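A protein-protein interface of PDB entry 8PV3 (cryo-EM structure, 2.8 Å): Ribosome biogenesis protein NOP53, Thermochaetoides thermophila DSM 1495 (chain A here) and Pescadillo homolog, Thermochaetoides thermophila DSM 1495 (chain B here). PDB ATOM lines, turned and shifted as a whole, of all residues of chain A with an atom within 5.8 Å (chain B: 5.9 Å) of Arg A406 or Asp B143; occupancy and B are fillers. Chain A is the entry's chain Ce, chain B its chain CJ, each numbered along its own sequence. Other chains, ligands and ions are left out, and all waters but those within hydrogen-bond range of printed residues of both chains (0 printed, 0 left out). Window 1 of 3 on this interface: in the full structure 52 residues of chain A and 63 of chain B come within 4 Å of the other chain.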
ATOM      1  N   ALA A 205      17.561 -20.936  11.413  1.00  0.00           N
ATOM      2  CA  ALA A 205      16.329 -21.708  11.291  1.00  0.00           C
ATOM      3  C   ALA A 205      16.126 -22.612  12.501  1.00  0.00           C
ATOM      4  O   ALA A 205      15.034 -22.662  13.078  1.00  0.00           O
ATOM      5  CB  ALA A 205      16.349 -22.525  10.000  1.00  0.00           C
ATOM      6  N   VAL A 206      17.169 -23.334  12.898  1.00  0.00           N
ATOM      7  CA  VAL A 206      17.150 -24.117  14.130  1.00  0.00           C
ATOM      8  C   VAL A 206      18.283 -23.616  15.017  1.00  0.00           C
ATOM      9  O   VAL A 206      19.447 -23.984  14.797  1.00  0.00           O
ATOM     10  CB  VAL A 206      17.280 -25.623  13.852  1.00  0.00           C
ATOM     11  CG1 VAL A 206      17.218 -26.407  15.152  1.00  0.00           C
ATOM     12  CG2 VAL A 206      16.191 -26.089  12.904  1.00  0.00           C
ATOM     13  N   ASN A 401       5.000 -26.089  21.295  1.00  0.00           N
ATOM     14  CA  ASN A 401       4.364 -26.652  20.112  1.00  0.00           C
ATOM     15  C   ASN A 401       5.280 -26.402  18.926  1.00  0.00           C
ATOM     16  O   ASN A 401       5.631 -25.252  18.648  1.00  0.00           O
ATOM     17  CB  ASN A 401       2.985 -26.032  19.875  1.00  0.00           C
ATOM     18  CG  ASN A 401       2.151 -26.827  18.895  1.00  0.00           C
ATOM     19  OD1 ASN A 401       2.450 -27.984  18.604  1.00  0.00           O
ATOM     20  ND2 ASN A 401       1.094 -26.210  18.383  1.00  0.00           N
ATOM     21  N   LEU A 402       5.664 -27.473  18.231  1.00  0.00           N
ATOM     22  CA  LEU A 402       6.661 -27.335  17.175  1.00  0.00           C
ATOM     23  C   LEU A 402       6.066 -26.714  15.916  1.00  0.00           C
ATOM     24  O   LEU A 402       6.785 -26.068  15.145  1.00  0.00           O
ATOM     25  CB  LEU A 402       7.298 -28.690  16.873  1.00  0.00           C
ATOM     26  CG  LEU A 402       8.152 -29.271  18.004  1.00  0.00           C
ATOM     27  CD1 LEU A 402       8.985 -30.430  17.502  1.00  0.00           C
ATOM     28  CD2 LEU A 402       9.045 -28.214  18.627  1.00  0.00           C
ATOM     29  N   LEU A 403       4.758 -26.884  15.696  1.00  0.00           N
ATOM     30  CA  LEU A 403       4.091 -26.159  14.616  1.00  0.00           C
ATOM     31  C   LEU A 403       4.188 -24.655  14.828  1.00  0.00           C
ATOM     32  O   LEU A 403       4.565 -23.909  13.914  1.00  0.00           O
ATOM     33  CB  LEU A 403       2.620 -26.566  14.510  1.00  0.00           C
ATOM     34  CG  LEU A 403       2.147 -27.813  13.756  1.00  0.00           C
ATOM     35  CD1 LEU A 403       2.465 -27.693  12.273  1.00  0.00           C
ATOM     36  CD2 LEU A 403       2.684 -29.110  14.339  1.00  0.00           C
ATOM     37  N   LYS A 404       3.870 -24.198  16.041  1.00  0.00           N
ATOM     38  CA  LYS A 404       3.964 -22.778  16.353  1.00  0.00           C
ATOM     39  C   LYS A 404       5.412 -22.314  16.352  1.00  0.00           C
ATOM     40  O   LYS A 404       5.700 -21.165  16.000  1.00  0.00           O
ATOM     41  CB  LYS A 404       3.301 -22.498  17.701  1.00  0.00           C
ATOM     42  CG  LYS A 404       2.957 -21.040  17.937  1.00  0.00           C
ATOM     43  CD  LYS A 404       2.112 -20.878  19.188  1.00  0.00           C
ATOM     44  CE  LYS A 404       1.640 -19.444  19.356  1.00  0.00           C
ATOM     45  NZ  LYS A 404       0.798 -19.279  20.572  1.00  0.00           N
ATOM     46  N   ASP A 405       6.340 -23.203  16.717  1.00  0.00           N
ATOM     47  CA  ASP A 405       7.759 -22.863  16.676  1.00  0.00           C
ATOM     48  C   ASP A 405       8.230 -22.614  15.247  1.00  0.00           C
ATOM     49  O   ASP A 405       8.916 -21.621  14.978  1.00  0.00           O
ATOM     50  CB  ASP A 405       8.575 -23.980  17.327  1.00  0.00           C
ATOM     51  CG  ASP A 405       9.964 -23.530  17.738  1.00  0.00           C
ATOM     52  OD1 ASP A 405      10.305 -22.349  17.520  1.00  0.00           O
ATOM     53  OD2 ASP A 405      10.716 -24.363  18.285  1.00  0.00           O
ATOM     54  N   ARG A 406       7.850 -23.490  14.312  1.00  0.00           N
ATOM     55  CA  ARG A 406       8.243 -23.299  12.919  1.00  0.00           C
ATOM     56  C   ARG A 406       7.550 -22.088  12.307  1.00  0.00           C
ATOM     57  O   ARG A 406       8.155 -21.353  11.515  1.00  0.00           O
ATOM     58  CB  ARG A 406       7.938 -24.557  12.104  1.00  0.00           C
ATOM     59  CG  ARG A 406       8.713 -25.790  12.538  1.00  0.00           C
ATOM     60  CD  ARG A 406       9.899 -26.083  11.633  1.00  0.00           C
ATOM     61  NE  ARG A 406      10.831 -24.964  11.552  1.00  0.00           N
ATOM     62  CZ  ARG A 406      11.808 -24.740  12.419  1.00  0.00           C
ATOM     63  NH1 ARG A 406      12.002 -25.530  13.461  1.00  0.00           N
ATOM     64  NH2 ARG A 406      12.607 -23.694  12.240  1.00  0.00           N
ATOM     65  N   TYR A 407       6.284 -21.859  12.669  1.00  0.00           N
ATOM     66  CA  TYR A 407       5.561 -20.692  12.172  1.00  0.00           C
ATOM     67  C   TYR A 407       6.202 -19.394  12.659  1.00  0.00           C
ATOM     68  O   TYR A 407       6.395 -18.451  11.875  1.00  0.00           O
ATOM     69  CB  TYR A 407       4.099 -20.785  12.608  1.00  0.00           C
ATOM     70  CG  TYR A 407       3.180 -19.734  12.038  1.00  0.00           C
ATOM     71  CD1 TYR A 407       3.012 -19.600  10.667  1.00  0.00           C
ATOM     72  CD2 TYR A 407       2.451 -18.898  12.872  1.00  0.00           C
ATOM     73  CE1 TYR A 407       2.162 -18.647  10.144  1.00  0.00           C
ATOM     74  CE2 TYR A 407       1.596 -17.945  12.357  1.00  0.00           C
ATOM     75  CZ  TYR A 407       1.457 -17.824  10.993  1.00  0.00           C
ATOM     76  OH  TYR A 407       0.610 -16.875  10.475  1.00  0.00           O
ATOM     77  N   ARG A 408       6.568 -19.340  13.944  1.00  0.00           N
ATOM     78  CA  ARG A 408       7.255 -18.172  14.479  1.00  0.00           C
ATOM     79  C   ARG A 408       8.629 -17.999  13.850  1.00  0.00           C
ATOM     80  O   ARG A 408       9.076 -16.868  13.637  1.00  0.00           O
ATOM     81  CB  ARG A 408       7.388 -18.279  15.996  1.00  0.00           C
ATOM     82  CG  ARG A 408       6.135 -17.935  16.765  1.00  0.00           C
ATOM     83  CD  ARG A 408       6.426 -17.927  18.253  1.00  0.00           C
ATOM     84  NE  ARG A 408       7.564 -17.072  18.567  1.00  0.00           N
ATOM     85  CZ  ARG A 408       7.467 -15.831  19.020  1.00  0.00           C
ATOM     86  NH1 ARG A 408       6.292 -15.266  19.242  1.00  0.00           N
ATOM     87  NH2 ARG A 408       8.577 -15.138  19.258  1.00  0.00           N
ATOM     88  N   SER A 409       9.322 -19.105  13.565  1.00  0.00           N
ATOM     89  CA  SER A 409      10.611 -19.018  12.885  1.00  0.00           C
ATOM     90  C   SER A 409      10.464 -18.398  11.504  1.00  0.00           C
ATOM     91  O   SER A 409      11.265 -17.538  11.115  1.00  0.00           O
ATOM     92  CB  SER A 409      11.242 -20.406  12.782  1.00  0.00           C
ATOM     93  OG  SER A 409      12.444 -20.364  12.035  1.00  0.00           O
ATOM     94  N   MET A 410       9.432 -18.809  10.759  1.00  0.00           N
ATOM     95  CA  MET A 410       9.183 -18.232   9.441  1.00  0.00           C
ATOM     96  C   MET A 410       8.868 -16.743   9.530  1.00  0.00           C
ATOM     97  O   MET A 410       9.393 -15.945   8.743  1.00  0.00           O
ATOM     98  CB  MET A 410       8.035 -18.965   8.748  1.00  0.00           C
ATOM     99  CG  MET A 410       8.310 -20.414   8.415  1.00  0.00           C
ATOM    100  SD  MET A 410       9.642 -20.637   7.231  1.00  0.00           S
ATOM    101  CE  MET A 410       9.814 -22.414   7.283  1.00  0.00           C
ATOM    102  N   ILE A 411       8.022 -16.349  10.487  1.00  0.00           N
ATOM    103  CA  ILE A 411       7.651 -14.938  10.607  1.00  0.00           C
ATOM    104  C   ILE A 411       8.849 -14.094  11.033  1.00  0.00           C
ATOM    105  O   ILE A 411       9.083 -13.008  10.491  1.00  0.00           O
ATOM    106  CB  ILE A 411       6.467 -14.763  11.574  1.00  0.00           C
ATOM    107  CG1 ILE A 411       5.246 -15.525  11.069  1.00  0.00           C
ATOM    108  CG2 ILE A 411       6.113 -13.292  11.729  1.00  0.00           C
ATOM    109  CD1 ILE A 411       4.044 -15.381  11.960  1.00  0.00           C
ATOM    110  N   ARG A 413      12.140 -14.766  10.679  1.00  0.00           N
ATOM    111  CA  ARG A 413      13.074 -14.666   9.569  1.00  0.00           C
ATOM    112  C   ARG A 413      12.501 -13.909   8.378  1.00  0.00           C
ATOM    113  O   ARG A 413      13.258 -13.549   7.472  1.00  0.00           O
ATOM    114  CB  ARG A 413      13.528 -16.058   9.133  1.00  0.00           C
ATOM    115  CG  ARG A 413      14.492 -16.706  10.108  1.00  0.00           C
ATOM    116  CD  ARG A 413      14.940 -18.053   9.599  1.00  0.00           C
ATOM    117  NE  ARG A 413      13.860 -19.026   9.675  1.00  0.00           N
ATOM    118  CZ  ARG A 413      13.713 -20.047   8.845  1.00  0.00           C
ATOM    119  NH1 ARG A 413      14.565 -20.261   7.855  1.00  0.00           N
ATOM    120  NH2 ARG A 413      12.684 -20.872   9.009  1.00  0.00           N
ATOM    121  N   LYS A 415      10.005 -14.663   6.024  1.00  0.00           N
ATOM    122  CA  LYS A 415       9.527 -15.284   4.798  1.00  0.00           C
ATOM    123  C   LYS A 415       8.038 -15.045   4.590  1.00  0.00           C
ATOM    124  O   LYS A 415       7.544 -15.185   3.466  1.00  0.00           O
ATOM    125  CB  LYS A 415       9.838 -16.778   4.817  1.00  0.00           C
ATOM    126  CG  LYS A 415      11.325 -17.073   4.895  1.00  0.00           C
ATOM    127  CD  LYS A 415      11.611 -18.559   4.897  1.00  0.00           C
ATOM    128  CE  LYS A 415      13.105 -18.820   4.913  1.00  0.00           C
ATOM    129  NZ  LYS A 415      13.417 -20.273   4.936  1.00  0.00           N
ATOM    130  N   ARG B 139      22.442 -26.317   3.158  1.00  0.00           N
ATOM    131  CA  ARG B 139      22.260 -25.290   4.174  1.00  0.00           C
ATOM    132  C   ARG B 139      20.797 -25.040   4.520  1.00  0.00           C
ATOM    133  O   ARG B 139      20.508 -24.692   5.669  1.00  0.00           O
ATOM    134  CB  ARG B 139      22.924 -23.985   3.729  1.00  0.00           C
ATOM    135  CG  ARG B 139      24.441 -24.044   3.769  1.00  0.00           C
ATOM    136  CD  ARG B 139      25.071 -22.803   3.173  1.00  0.00           C
ATOM    137  NE  ARG B 139      26.524 -22.915   3.125  1.00  0.00           N
ATOM    138  CZ  ARG B 139      27.326 -22.021   2.564  1.00  0.00           C
ATOM    139  NH1 ARG B 139      26.850 -20.929   1.992  1.00  0.00           N
ATOM    140  NH2 ARG B 139      28.640 -22.230   2.577  1.00  0.00           N
ATOM    141  N   ASP B 140      19.870 -25.205   3.576  1.00  0.00           N
ATOM    142  CA  ASP B 140      18.448 -25.113   3.896  1.00  0.00           C
ATOM    143  C   ASP B 140      17.867 -26.443   4.369  1.00  0.00           C
ATOM    144  O   ASP B 140      16.692 -26.499   4.773  1.00  0.00           O
ATOM    145  CB  ASP B 140      17.655 -24.592   2.699  1.00  0.00           C
ATOM    146  CG  ASP B 140      16.451 -23.769   3.118  1.00  0.00           C
ATOM    147  OD1 ASP B 140      16.567 -23.008   4.102  1.00  0.00           O
ATOM    148  OD2 ASP B 140      15.389 -23.890   2.474  1.00  0.00           O
ATOM    149  N   LEU B 141      18.667 -27.514   4.325  1.00  0.00           N
ATOM    150  CA  LEU B 141      18.222 -28.808   4.831  1.00  0.00           C
ATOM    151  C   LEU B 141      17.846 -28.796   6.306  1.00  0.00           C
ATOM    152  O   LEU B 141      17.075 -29.657   6.719  1.00  0.00           O
ATOM    153  CB  LEU B 141      19.291 -29.877   4.619  1.00  0.00           C
ATOM    154  CG  LEU B 141      19.172 -30.731   3.362  1.00  0.00           C
ATOM    155  CD1 LEU B 141      20.105 -31.917   3.473  1.00  0.00           C
ATOM    156  CD2 LEU B 141      17.741 -31.187   3.158  1.00  0.00           C
ATOM    157  N   ASP B 142      18.360 -27.855   7.103  1.00  0.00           N
ATOM    158  CA  ASP B 142      17.980 -27.790   8.512  1.00  0.00           C
ATOM    159  C   ASP B 142      16.483 -27.542   8.661  1.00  0.00           C
ATOM    160  O   ASP B 142      15.762 -28.324   9.301  1.00  0.00           O
ATOM    161  CB  ASP B 142      18.772 -26.679   9.204  1.00  0.00           C
ATOM    162  CG  ASP B 142      20.258 -26.970   9.262  1.00  0.00           C
ATOM    163  OD1 ASP B 142      20.761 -27.341  10.341  1.00  0.00           O
ATOM    164  OD2 ASP B 142      20.930 -26.822   8.221  1.00  0.00           O
ATOM    165  N   ASP B 143      15.992 -26.485   8.011  1.00  0.00           N
ATOM    166  CA  ASP B 143      14.569 -26.172   8.028  1.00  0.00           C
ATOM    167  C   ASP B 143      13.763 -27.233   7.293  1.00  0.00           C
ATOM    168  O   ASP B 143      12.657 -27.584   7.721  1.00  0.00           O
ATOM    169  CB  ASP B 143      14.335 -24.797   7.412  1.00  0.00           C
ATOM    170  CG  ASP B 143      13.167 -24.074   8.035  1.00  0.00           C
ATOM    171  OD1 ASP B 143      12.409 -24.709   8.799  1.00  0.00           O
ATOM    172  OD2 ASP B 143      13.010 -22.869   7.765  1.00  0.00           O
ATOM    173  N   CYS B 144      14.307 -27.757   6.185  1.00  0.00           N
ATOM    174  CA  CYS B 144      13.611 -28.800   5.430  1.00  0.00           C
ATOM    175  C   CYS B 144      13.360 -30.044   6.281  1.00  0.00           C
ATOM    176  O   CYS B 144      12.235 -30.562   6.339  1.00  0.00           O
ATOM    177  CB  CYS B 144      14.423 -29.159   4.185  1.00  0.00           C
ATOM    178  SG  CYS B 144      13.800 -30.571   3.252  1.00  0.00           S
ATOM    179  N   LEU B 145      14.397 -30.516   6.975  1.00  0.00           N
ATOM    180  CA  LEU B 145      14.284 -31.716   7.791  1.00  0.00           C
ATOM    181  C   LEU B 145      13.407 -31.483   9.009  1.00  0.00           C
ATOM    182  O   LEU B 145      12.632 -32.366   9.384  1.00  0.00           O
ATOM    183  CB  LEU B 145      15.668 -32.193   8.217  1.00  0.00           C
ATOM    184  CG  LEU B 145      16.551 -32.806   7.135  1.00  0.00           C
ATOM    185  CD1 LEU B 145      17.964 -32.905   7.657  1.00  0.00           C
ATOM    186  CD2 LEU B 145      16.030 -34.162   6.722  1.00  0.00           C
ATOM    187  N   SER B 146      13.512 -30.305   9.639  1.00  0.00           N
ATOM    188  CA  SER B 146      12.635 -30.008  10.771  1.00  0.00           C
ATOM    189  C   SER B 146      11.171 -30.007  10.347  1.00  0.00           C
ATOM    190  O   SER B 146      10.323 -30.618  11.013  1.00  0.00           O
ATOM    191  CB  SER B 146      13.012 -28.664  11.389  1.00  0.00           C
ATOM    192  OG  SER B 146      14.321 -28.700  11.926  1.00  0.00           O
ATOM    193  N   MET B 147      10.876 -29.385   9.201  1.00  0.00           N
ATOM    194  CA  MET B 147       9.512 -29.307   8.690  1.00  0.00           C
ATOM    195  C   MET B 147       8.959 -30.694   8.379  1.00  0.00           C
ATOM    196  O   MET B 147       7.843 -31.041   8.792  1.00  0.00           O
ATOM    197  CB  MET B 147       9.508 -28.443   7.430  1.00  0.00           C
ATOM    198  CG  MET B 147       8.149 -28.153   6.845  1.00  0.00           C
ATOM    199  SD  MET B 147       7.183 -27.181   7.999  1.00  0.00           S
ATOM    200  CE  MET B 147       8.023 -25.611   7.852  1.00  0.00           C
ATOM    201  N   LEU B 148       9.744 -31.516   7.674  1.00  0.00           N
ATOM    202  CA  LEU B 148       9.233 -32.814   7.246  1.00  0.00           C
ATOM    203  C   LEU B 148       9.153 -33.801   8.403  1.00  0.00           C
ATOM    204  O   LEU B 148       8.223 -34.612   8.463  1.00  0.00           O
ATOM    205  CB  LEU B 148      10.085 -33.372   6.109  1.00  0.00           C
ATOM    206  CG  LEU B 148       9.919 -32.650   4.769  1.00  0.00           C
ATOM    207  CD1 LEU B 148      10.516 -33.467   3.652  1.00  0.00           C
ATOM    208  CD2 LEU B 148       8.458 -32.348   4.480  1.00  0.00           C
ATOM    209  N   LEU B 150       8.497 -32.940  11.417  1.00  0.00           N
ATOM    210  CA  LEU B 150       7.321 -32.532  12.176  1.00  0.00           C
ATOM    211  C   LEU B 150       6.041 -33.034  11.515  1.00  0.00           C
ATOM    212  O   LEU B 150       5.163 -33.591  12.182  1.00  0.00           O
ATOM    213  CB  LEU B 150       7.298 -31.012  12.319  1.00  0.00           C
ATOM    214  CG  LEU B 150       6.063 -30.405  12.979  1.00  0.00           C
ATOM    215  CD1 LEU B 150       5.844 -31.021  14.350  1.00  0.00           C
ATOM    216  CD2 LEU B 150       6.209 -28.900  13.076  1.00  0.00           C
ATOM    217  N   LEU B 207      21.703 -29.366  11.681  1.00  0.00           N
ATOM    218  CA  LEU B 207      21.050 -29.590  12.963  1.00  0.00           C
ATOM    219  C   LEU B 207      19.546 -29.433  12.801  1.00  0.00           C
ATOM    220  O   LEU B 207      19.074 -28.387  12.347  1.00  0.00           O
ATOM    221  CB  LEU B 207      21.574 -28.612  14.015  1.00  0.00           C
ATOM    222  CG  LEU B 207      20.788 -28.526  15.321  1.00  0.00           C
ATOM    223  CD1 LEU B 207      20.978 -29.781  16.144  1.00  0.00           C
ATOM    224  CD2 LEU B 207      21.206 -27.302  16.110  1.00  0.00           C
ATOM    225  N   LEU B 209      15.411 -30.726  14.470  1.00  0.00           N
ATOM    226  CA  LEU B 209      14.658 -31.098  15.658  1.00  0.00           C
ATOM    227  C   LEU B 209      13.545 -32.065  15.279  1.00  0.00           C
ATOM    228  O   LEU B 209      12.814 -31.831  14.311  1.00  0.00           O
ATOM    229  CB  LEU B 209      14.075 -29.856  16.332  1.00  0.00           C
ATOM    230  CG  LEU B 209      13.295 -30.055  17.628  1.00  0.00           C
ATOM    231  CD1 LEU B 209      14.119 -30.843  18.618  1.00  0.00           C
ATOM    232  CD2 LEU B 209      12.900 -28.715  18.210  1.00  0.00           C
ATOM    233  N   MET B 227       1.710 -23.535   5.848  1.00  0.00           N
ATOM    234  CA  MET B 227       2.646 -24.551   6.320  1.00  0.00           C
ATOM    235  C   MET B 227       2.660 -25.752   5.384  1.00  0.00           C
ATOM    236  O   MET B 227       3.720 -26.313   5.097  1.00  0.00           O
ATOM    237  CB  MET B 227       2.289 -24.984   7.743  1.00  0.00           C
ATOM    238  CG  MET B 227       2.446 -23.894   8.792  1.00  0.00           C
ATOM    239  SD  MET B 227       4.126 -23.272   8.950  1.00  0.00           S
ATOM    240  CE  MET B 227       4.926 -24.696   9.673  1.00  0.00           C
ATOM    241  N   TYR B 234       9.483 -28.338   0.601  1.00  0.00           N
ATOM    242  CA  TYR B 234      10.568 -29.057   1.255  1.00  0.00           C
ATOM    243  C   TYR B 234      10.598 -30.526   0.857  1.00  0.00           C
ATOM    244  O   TYR B 234      11.678 -31.119   0.783  1.00  0.00           O
ATOM    245  CB  TYR B 234      10.453 -28.897   2.767  1.00  0.00           C
ATOM    246  CG  TYR B 234      10.883 -27.529   3.242  1.00  0.00           C
ATOM    247  CD1 TYR B 234      11.985 -26.895   2.684  1.00  0.00           C
ATOM    248  CD2 TYR B 234      10.180 -26.866   4.234  1.00  0.00           C
ATOM    249  CE1 TYR B 234      12.378 -25.644   3.109  1.00  0.00           C
ATOM    250  CE2 TYR B 234      10.565 -25.617   4.666  1.00  0.00           C
ATOM    251  CZ  TYR B 234      11.664 -25.010   4.101  1.00  0.00           C
ATOM    252  OH  TYR B 234      12.046 -23.764   4.533  1.00  0.00           O
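Among the printed residues, merely in contact across the chains: Ala A205 with Asp B143 (3.99 Å), Val A206 with Ser B146 (3.4 Å), Val A206 with Leu B207 (3.6 Å), Leu A402 with Leu B150 (3.6 Å), Leu A402 with Leu B209 (3.9 Å), Leu A403 with Leu B150 (3.6 Å), Arg A406 with Ser B146 (3.9 Å), Arg A406 with Met B227 (3.9 Å), Met A410 with Asp B143 (3.3 Å), Met A410 with Met B147 (3.7 Å), Met A410 with Tyr B234 (3.8 Å) and Lys A415 with Tyr B234 (3.8 Å).
Of the 15 printed residues of chain B, 8 touch a printed residue of chain A. Printed residues of chain A that touch a printed residue of chain B: Ala A205, Val A206, Leu A402, Leu A403, Arg A406, Met A410, Arg A413 and Lys A415. Along chain A the printed residues that touch a printed residue of chain B span positions 205 to 415. Among the printed residues, Asp or Glu carboxylates within 4 Å of a Lys or Arg side-chain nitrogen of the other chain: Arg A406 with Asp B143 (3.2 Å), Arg A413 with Asp B143 (2.4 Å) and Lys A415 with Asp B143 (3.9 Å).
Arg A406 touches just these residues of chain B: Asp B143 (3.2 Å), Ser B146 (3.9 Å) and Met B227 (3.9 Å). Of the printed residues of chain A, Asp B143 touches Ala A205 (3.99 Å), Arg A406 (3.2 Å), Met A410 (3.3 Å), Arg A413 (2.4 Å) and Lys A415 (3.9 Å). Of the printed residues of chain B, Val A206 touches Ser B146 (3.4 Å) and Leu B207 (3.6 Å). Printed residues of chain A within 4 Å of Leu B207: Val A206 (3.6 Å). Printed residues of chain B within 4 Å of Arg A413: Asp B143 (2.4 Å). Of the printed residues of chain A, Met B147 touches Met A410. Lys A404 touches none of the printed residues of chain B. The nearest residue of chain B that does not touch Arg A406 is Leu B150 (4.03 Å).
The side-chain sulfur (SG) of Cys B144 is in hydrogen-bond range of the backbone carbonyl oxygen (O) of Tyr B234, at 3.3 Å. The side-chain hydroxyl of Ser A409 lies within hydrogen-bond range of the guanidinium group of Arg A406. OG of Ser B146 lies within hydrogen-bond range of N of Leu B209. The side-chain hydroxyl (OG) of Ser A409 is in hydrogen-bond range of the guanidinium group (NE) of Arg A413, 3.1 Å away. The backbone carbonyl oxygen (O) of Asp B142 sits at hydrogen-bond distance from the side-chain hydroxyl (OG) of Ser B146 (3.0 Å). O of Ala A205 sits at hydrogen-bond distance from NH2 of Arg A406 (2.8 Å).
The side-chain carboxylate (OD2) of Asp B143 lies within salt-bridge range of the guanidinium group (NH1) of Arg A413 (3.0 Å). The side-chain carboxylate (OD1) of Asp B143 is in salt-bridge range of the guanidinium group (NE) of Arg A406. NZ of Lys A415 is in salt-bridge range of OD2 of Asp B143, 3.9 Å away.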
